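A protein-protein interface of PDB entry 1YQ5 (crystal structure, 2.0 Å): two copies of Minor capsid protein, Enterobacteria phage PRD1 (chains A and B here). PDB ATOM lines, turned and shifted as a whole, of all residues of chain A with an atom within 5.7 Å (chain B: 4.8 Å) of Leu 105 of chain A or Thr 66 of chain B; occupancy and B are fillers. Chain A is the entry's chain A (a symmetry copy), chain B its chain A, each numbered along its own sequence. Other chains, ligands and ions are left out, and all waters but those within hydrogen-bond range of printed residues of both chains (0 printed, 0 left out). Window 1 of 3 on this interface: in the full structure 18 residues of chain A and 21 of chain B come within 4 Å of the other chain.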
ATOM      1  N   TYR A  61      14.444  23.999 -13.561  1.00  0.00           N
ATOM      2  CA  TYR A  61      15.173  22.830 -14.023  1.00  0.00           C
ATOM      3  C   TYR A  61      16.048  23.114 -15.232  1.00  0.00           C
ATOM      4  O   TYR A  61      15.613  23.763 -16.183  1.00  0.00           O
ATOM      5  CB  TYR A  61      14.196  21.708 -14.384  1.00  0.00           C
ATOM      6  CG  TYR A  61      13.539  21.062 -13.190  1.00  0.00           C
ATOM      7  CD1 TYR A  61      12.499  21.696 -12.509  1.00  0.00           C
ATOM      8  CD2 TYR A  61      13.988  19.831 -12.713  1.00  0.00           C
ATOM      9  CE1 TYR A  61      11.925  21.112 -11.376  1.00  0.00           C
ATOM     10  CE2 TYR A  61      13.426  19.244 -11.590  1.00  0.00           C
ATOM     11  CZ  TYR A  61      12.399  19.885 -10.922  1.00  0.00           C
ATOM     12  OH  TYR A  61      11.866  19.301  -9.792  1.00  0.00           O
ATOM     13  N   GLN A  62      17.285  22.627 -15.178  1.00  0.00           N
ATOM     14  CA  GLN A  62      18.219  22.775 -16.287  1.00  0.00           C
ATOM     15  C   GLN A  62      18.177  21.428 -16.992  1.00  0.00           C
ATOM     16  O   GLN A  62      18.406  20.385 -16.376  1.00  0.00           O
ATOM     17  CB  GLN A  62      19.635  23.063 -15.785  1.00  0.00           C
ATOM     18  CG  GLN A  62      20.691  23.091 -16.892  1.00  0.00           C
ATOM     19  CD  GLN A  62      20.336  24.031 -18.036  1.00  0.00           C
ATOM     20  OE1 GLN A  62      20.035  25.206 -17.821  1.00  0.00           O
ATOM     21  NE2 GLN A  62      20.378  23.514 -19.263  1.00  0.00           N
ATOM     22  N   ILE A  63      17.882  21.456 -18.284  1.00  0.00           N
ATOM     23  CA  ILE A  63      17.749  20.241 -19.068  1.00  0.00           C
ATOM     24  C   ILE A  63      18.570  20.259 -20.349  1.00  0.00           C
ATOM     25  O   ILE A  63      18.643  21.278 -21.043  1.00  0.00           O
ATOM     26  CB  ILE A  63      16.273  20.038 -19.446  1.00  0.00           C
ATOM     27  CG1 ILE A  63      15.425  19.967 -18.173  1.00  0.00           C
ATOM     28  CG2 ILE A  63      16.109  18.794 -20.299  1.00  0.00           C
ATOM     29  CD1 ILE A  63      13.956  20.244 -18.406  1.00  0.00           C
ATOM     30  N   THR A  64      19.178  19.120 -20.661  1.00  0.00           N
ATOM     31  CA  THR A  64      19.965  18.981 -21.875  1.00  0.00           C
ATOM     32  C   THR A  64      19.753  17.610 -22.492  1.00  0.00           C
ATOM     33  O   THR A  64      19.730  16.598 -21.794  1.00  0.00           O
ATOM     34  CB  THR A  64      21.486  19.135 -21.618  1.00  0.00           C
ATOM     35  OG1 THR A  64      21.783  20.487 -21.250  1.00  0.00           O
ATOM     36  CG2 THR A  64      22.281  18.771 -22.879  1.00  0.00           C
ATOM     37  N   VAL A  81      11.486  18.775 -26.197  1.00  0.00           N
ATOM     38  CA  VAL A  81      11.314  18.509 -24.777  1.00  0.00           C
ATOM     39  C   VAL A  81       9.957  19.088 -24.411  1.00  0.00           C
ATOM     40  O   VAL A  81       9.630  20.207 -24.812  1.00  0.00           O
ATOM     41  CB  VAL A  81      12.373  19.222 -23.915  1.00  0.00           C
ATOM     42  CG1 VAL A  81      12.061  19.011 -22.437  1.00  0.00           C
ATOM     43  CG2 VAL A  81      13.758  18.697 -24.244  1.00  0.00           C
ATOM     44  N   PHE A  88       9.272  22.556 -26.187  1.00  0.00           N
ATOM     45  CA  PHE A  88      10.423  23.330 -26.635  1.00  0.00           C
ATOM     46  C   PHE A  88      11.139  22.550 -27.721  1.00  0.00           C
ATOM     47  O   PHE A  88      11.388  21.351 -27.574  1.00  0.00           O
ATOM     48  CB  PHE A  88      11.358  23.590 -25.456  1.00  0.00           C
ATOM     49  CG  PHE A  88      10.640  24.045 -24.213  1.00  0.00           C
ATOM     50  CD1 PHE A  88      10.215  23.124 -23.263  1.00  0.00           C
ATOM     51  CD2 PHE A  88      10.357  25.391 -24.012  1.00  0.00           C
ATOM     52  CE1 PHE A  88       9.515  23.537 -22.129  1.00  0.00           C
ATOM     53  CE2 PHE A  88       9.658  25.814 -22.884  1.00  0.00           C
ATOM     54  CZ  PHE A  88       9.238  24.881 -21.939  1.00  0.00           C
ATOM     55  N   ILE A 103      19.935  20.261 -27.540  1.00  0.00           N
ATOM     56  CA  ILE A 103      18.906  21.163 -27.044  1.00  0.00           C
ATOM     57  C   ILE A 103      19.111  21.266 -25.539  1.00  0.00           C
ATOM     58  O   ILE A 103      19.207  20.251 -24.841  1.00  0.00           O
ATOM     59  CB  ILE A 103      17.453  20.694 -27.350  1.00  0.00           C
ATOM     60  CG1 ILE A 103      16.482  21.837 -27.009  1.00  0.00           C
ATOM     61  CG2 ILE A 103      17.093  19.452 -26.542  1.00  0.00           C
ATOM     62  CD1 ILE A 103      15.035  21.594 -27.427  1.00  0.00           C
ATOM     63  N   SER A 104      19.221  22.496 -25.052  1.00  0.00           N
ATOM     64  CA  SER A 104      19.422  22.746 -23.634  1.00  0.00           C
ATOM     65  C   SER A 104      18.431  23.800 -23.200  1.00  0.00           C
ATOM     66  O   SER A 104      18.207  24.780 -23.911  1.00  0.00           O
ATOM     67  CB  SER A 104      20.848  23.217 -23.366  1.00  0.00           C
ATOM     68  OG  SER A 104      21.752  22.146 -23.565  1.00  0.00           O
ATOM     69  N   LEU A 105      17.857  23.602 -22.020  1.00  0.00           N
ATOM     70  CA  LEU A 105      16.835  24.501 -21.517  1.00  0.00           C
ATOM     71  C   LEU A 105      16.846  24.700 -20.010  1.00  0.00           C
ATOM     72  O   LEU A 105      17.133  23.776 -19.252  1.00  0.00           O
ATOM     73  CB  LEU A 105      15.458  23.943 -21.890  1.00  0.00           C
ATOM     74  CG  LEU A 105      15.186  23.561 -23.341  1.00  0.00           C
ATOM     75  CD1 LEU A 105      14.294  22.325 -23.391  1.00  0.00           C
ATOM     76  CD2 LEU A 105      14.539  24.733 -24.057  1.00  0.00           C
ATOM     77  N   LEU A 106      16.533  25.920 -19.593  1.00  0.00           N
ATOM     78  CA  LEU A 106      16.386  26.253 -18.182  1.00  0.00           C
ATOM     79  C   LEU A 106      14.925  26.681 -18.175  1.00  0.00           C
ATOM     80  O   LEU A 106      14.572  27.682 -18.793  1.00  0.00           O
ATOM     81  CB  LEU A 106      17.267  27.435 -17.762  1.00  0.00           C
ATOM     82  CG  LEU A 106      16.922  27.961 -16.356  1.00  0.00           C
ATOM     83  CD1 LEU A 106      17.094  26.845 -15.345  1.00  0.00           C
ATOM     84  CD2 LEU A 106      17.802  29.153 -15.990  1.00  0.00           C
ATOM     85  N   ILE A 107      14.077  25.913 -17.501  1.00  0.00           N
ATOM     86  CA  ILE A 107      12.655  26.213 -17.469  1.00  0.00           C
ATOM     87  C   ILE A 107      12.068  26.059 -16.077  1.00  0.00           C
ATOM     88  O   ILE A 107      12.668  25.428 -15.202  1.00  0.00           O
ATOM     89  CB  ILE A 107      11.883  25.263 -18.405  1.00  0.00           C
ATOM     90  CG1 ILE A 107      12.094  23.813 -17.947  1.00  0.00           C
ATOM     91  CG2 ILE A 107      12.353  25.438 -19.836  1.00  0.00           C
ATOM     92  CD1 ILE A 107      11.286  22.781 -18.719  1.00  0.00           C
ATOM     93  N   THR B  64      17.794  31.273 -20.815  1.00  0.00           N
ATOM     94  CA  THR B  64      17.116  30.502 -21.845  1.00  0.00           C
ATOM     95  C   THR B  64      15.942  31.283 -22.407  1.00  0.00           C
ATOM     96  O   THR B  64      15.181  31.904 -21.666  1.00  0.00           O
ATOM     97  CB  THR B  64      16.557  29.160 -21.310  1.00  0.00           C
ATOM     98  OG1 THR B  64      17.637  28.281 -20.975  1.00  0.00           O
ATOM     99  CG2 THR B  64      15.674  28.487 -22.370  1.00  0.00           C
ATOM    100  N   MET B  65      15.818  31.272 -23.725  1.00  0.00           N
ATOM    101  CA  MET B  65      14.697  31.912 -24.381  1.00  0.00           C
ATOM    102  C   MET B  65      14.219  30.937 -25.434  1.00  0.00           C
ATOM    103  O   MET B  65      15.005  30.468 -26.260  1.00  0.00           O
ATOM    104  CB  MET B  65      15.084  33.230 -25.046  1.00  0.00           C
ATOM    105  CG  MET B  65      13.932  33.776 -25.885  1.00  0.00           C
ATOM    106  SD  MET B  65      14.177  35.562 -26.558  1.00  0.00           S
ATOM    107  CE  MET B  65      15.843  35.238 -27.539  1.00  0.00           C
ATOM    108  N   THR B  66      12.931  30.619 -25.387  1.00  0.00           N
ATOM    109  CA  THR B  66      12.337  29.690 -26.332  1.00  0.00           C
ATOM    110  C   THR B  66      11.115  30.301 -26.994  1.00  0.00           C
ATOM    111  O   THR B  66      10.506  31.231 -26.465  1.00  0.00           O
ATOM    112  CB  THR B  66      11.889  28.394 -25.633  1.00  0.00           C
ATOM    113  OG1 THR B  66      10.987  28.720 -24.568  1.00  0.00           O
ATOM    114  CG2 THR B  66      13.088  27.648 -25.072  1.00  0.00           C
ATOM    115  N   VAL B  67      10.760  29.771 -28.157  1.00  0.00           N
ATOM    116  CA  VAL B  67       9.591  30.251 -28.868  1.00  0.00           C
ATOM    117  C   VAL B  67       8.920  29.143 -29.657  1.00  0.00           C
ATOM    118  O   VAL B  67       9.582  28.263 -30.209  1.00  0.00           O
ATOM    119  CB  VAL B  67       9.932  31.392 -29.866  1.00  0.00           C
ATOM    120  CG1 VAL B  67      10.921  30.901 -30.913  1.00  0.00           C
ATOM    121  CG2 VAL B  67       8.659  31.877 -30.551  1.00  0.00           C
ATOM    122  N   LYS B  68       7.594  29.196 -29.667  1.00  0.00           N
ATOM    123  CA  LYS B  68       6.760  28.288 -30.432  1.00  0.00           C
ATOM    124  C   LYS B  68       5.746  29.211 -31.103  1.00  0.00           C
ATOM    125  O   LYS B  68       5.147  30.066 -30.449  1.00  0.00           O
ATOM    126  CB  LYS B  68       6.007  27.287 -29.540  1.00  0.00           C
ATOM    127  CG  LYS B  68       6.832  26.138 -28.967  1.00  0.00           C
ATOM    128  CD  LYS B  68       7.627  25.392 -30.037  1.00  0.00           C
ATOM    129  CE  LYS B  68       6.769  24.933 -31.221  1.00  0.00           C
ATOM    130  NZ  LYS B  68       5.699  23.950 -30.870  1.00  0.00           N
ATOM    131  N   GLY B 101      12.165  27.872 -31.938  1.00  0.00           N
ATOM    132  CA  GLY B 101      13.587  27.757 -31.700  1.00  0.00           C
ATOM    133  C   GLY B 101      13.939  27.873 -30.234  1.00  0.00           C
ATOM    134  O   GLY B 101      13.077  28.117 -29.386  1.00  0.00           O
ATOM    135  N   THR B 102      15.224  27.723 -29.944  1.00  0.00           N
ATOM    136  CA  THR B 102      15.710  27.774 -28.578  1.00  0.00           C
ATOM    137  C   THR B 102      17.129  28.316 -28.504  1.00  0.00           C
ATOM    138  O   THR B 102      17.954  28.026 -29.366  1.00  0.00           O
ATOM    139  CB  THR B 102      15.734  26.353 -27.958  1.00  0.00           C
ATOM    140  OG1 THR B 102      14.401  25.827 -27.890  1.00  0.00           O
ATOM    141  CG2 THR B 102      16.358  26.387 -26.566  1.00  0.00           C
ATOM    142  N   SER B 104      20.043  28.950 -25.313  1.00  0.00           N
ATOM    143  CA  SER B 104      20.372  28.847 -23.900  1.00  0.00           C
ATOM    144  C   SER B 104      21.824  29.228 -23.730  1.00  0.00           C
ATOM    145  O   SER B 104      22.674  28.834 -24.529  1.00  0.00           O
ATOM    146  CB  SER B 104      20.133  27.429 -23.393  1.00  0.00           C
ATOM    147  OG  SER B 104      18.744  27.163 -23.348  1.00  0.00           O
ATOM    148  N   LEU B 124      13.902  38.023 -31.082  1.00  0.00           N
ATOM    149  CA  LEU B 124      13.815  36.883 -31.982  1.00  0.00           C
ATOM    150  C   LEU B 124      12.804  37.208 -33.072  1.00  0.00           C
ATOM    151  O   LEU B 124      12.036  38.166 -32.954  1.00  0.00           O
ATOM    152  CB  LEU B 124      13.398  35.616 -31.214  1.00  0.00           C
ATOM    153  CG  LEU B 124      12.028  35.521 -30.535  1.00  0.00           C
ATOM    154  CD1 LEU B 124      10.921  35.408 -31.583  1.00  0.00           C
ATOM    155  CD2 LEU B 124      12.005  34.296 -29.630  1.00  0.00           C
ATOM    156  N   ILE B 135       4.426  31.939 -28.351  1.00  0.00           N
ATOM    157  CA  ILE B 135       4.513  31.739 -26.917  1.00  0.00           C
ATOM    158  C   ILE B 135       6.014  31.745 -26.687  1.00  0.00           C
ATOM    159  O   ILE B 135       6.727  30.833 -27.111  1.00  0.00           O
ATOM    160  CB  ILE B 135       3.931  30.398 -26.452  1.00  0.00           C
ATOM    161  CG1 ILE B 135       2.413  30.394 -26.638  1.00  0.00           C
ATOM    162  CG2 ILE B 135       4.254  30.194 -24.965  1.00  0.00           C
ATOM    163  CD1 ILE B 135       1.709  31.474 -25.830  1.00  0.00           C
ATOM    164  N   ILE B 136       6.489  32.807 -26.052  1.00  0.00           N
ATOM    165  CA  ILE B 136       7.901  32.962 -25.776  1.00  0.00           C
ATOM    166  C   ILE B 136       8.138  32.879 -24.278  1.00  0.00           C
ATOM    167  O   ILE B 136       7.426  33.505 -23.486  1.00  0.00           O
ATOM    168  CB  ILE B 136       8.416  34.326 -26.301  1.00  0.00           C
ATOM    169  CG1 ILE B 136       8.262  34.377 -27.823  1.00  0.00           C
ATOM    170  CG2 ILE B 136       9.876  34.537 -25.896  1.00  0.00           C
ATOM    171  CD1 ILE B 136       8.630  35.718 -28.433  1.00  0.00           C
ATOM    172  N   ASN B 137       9.121  32.078 -23.894  1.00  0.00           N
ATOM    173  CA  ASN B 137       9.478  31.932 -22.494  1.00  0.00           C
ATOM    174  C   ASN B 137      10.916  32.385 -22.337  1.00  0.00           C
ATOM    175  O   ASN B 137      11.790  31.991 -23.112  1.00  0.00           O
ATOM    176  CB  ASN B 137       9.332  30.478 -22.048  1.00  0.00           C
ATOM    177  CG  ASN B 137       7.884  30.082 -21.839  1.00  0.00           C
ATOM    178  OD1 ASN B 137       7.271  30.428 -20.822  1.00  0.00           O
ATOM    179  ND2 ASN B 137       7.326  29.368 -22.801  1.00  0.00           N
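OG of Ser 104 of chain B is in hydrogen-bond range of O of Ser 104 of chain A (2.5 Å).
The side-chain hydroxyl (OG1) of Thr 64 of chain B sits at hydrogen-bond distance from the backbone NH (N) of Leu 106 of chain A, at 3.0 Å.
Ser 104 of chain A touches its own counterpart, Ser 104 of chain B.
Positions printed for both chains: 64 and 104.
Of the 8 pairs that touch across the chains among the printed residues, 1 has its exchanged pair printed and touching as well.
Of the 12 printed residues of chain B, 4 touch a printed residue of chain A.
Among the printed residues, 8 pairs touch across the chains.
O of Asn 137 of chain B lies within hydrogen-bond range of N of Thr 66 of chain B.
N of Ile 63 of chain A sits at hydrogen-bond distance from O of Leu 105 of chain A, at 2.6 Å.
The side-chain amide nitrogen (NE2) of Gln 62 of chain A lies within hydrogen-bond range of the backbone carbonyl oxygen (O) of Leu 105 of chain A, at 3.3 Å.
The side-chain hydroxyl (OG1) of Thr 64 of chain B lies within hydrogen-bond range of the side-chain hydroxyl (OG) of Ser 104 of chain B (2.8 Å).
The side-chain hydroxyl of Ser 104 of chain A is in hydrogen-bond range of the side-chain hydroxyl of Thr 64 of chain A (2.8 Å).
N of Phe 88 of chain A lies within hydrogen-bond range of O of Val 81 of chain A, at 2.7 Å.
Phe 88 of chain A touches Thr 66 of chain B.
Thr 102 of chain B touches Ser 104 of chain A.
C of Leu 105 of chain A touches OG1 of Thr 64 of chain B (3.8 Å).
CG2 of Thr 66 of chain B touches CD2 of Leu 105 of chain A (3.4 Å).
CG2 of Thr 102 of chain B touches CD2 of Leu 105 of chain A (3.5 Å).
CA of Leu 105 of chain A touches OG of Ser 104 of chain B, at 3.8 Å.
Of chain B, only Thr 64 (3.8 Å), Thr 66 (3.4 Å), Thr 102 (3.5 Å) and Ser 104 (3.8 Å) come within 4 Å of Leu 105 of chain A.
Thr 66 of chain B touches two residues of chain A.
Of the printed residues of chain A, Thr 102 of chain B touches Ser 104 and Leu 105.
Of the printed residues of chain B, Phe 88 of chain A touches Thr 66.
Of the printed residues of chain A, Thr 64 of chain B touches Leu 105 and Leu 106.
Of the printed residues of chain B, Leu 106 of chain A touches Thr 64 (3.0 Å).
Printed residues of chain A within 4 Å of Ser 104 of chain B: Ser 104 and Leu 105.
Tyr 61 of chain A touches none of the printed residues of chain B.
The nearest printed residue of chain B that does not touch Leu 105 of chain A is Met 65 of chain B (6.2 Å).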
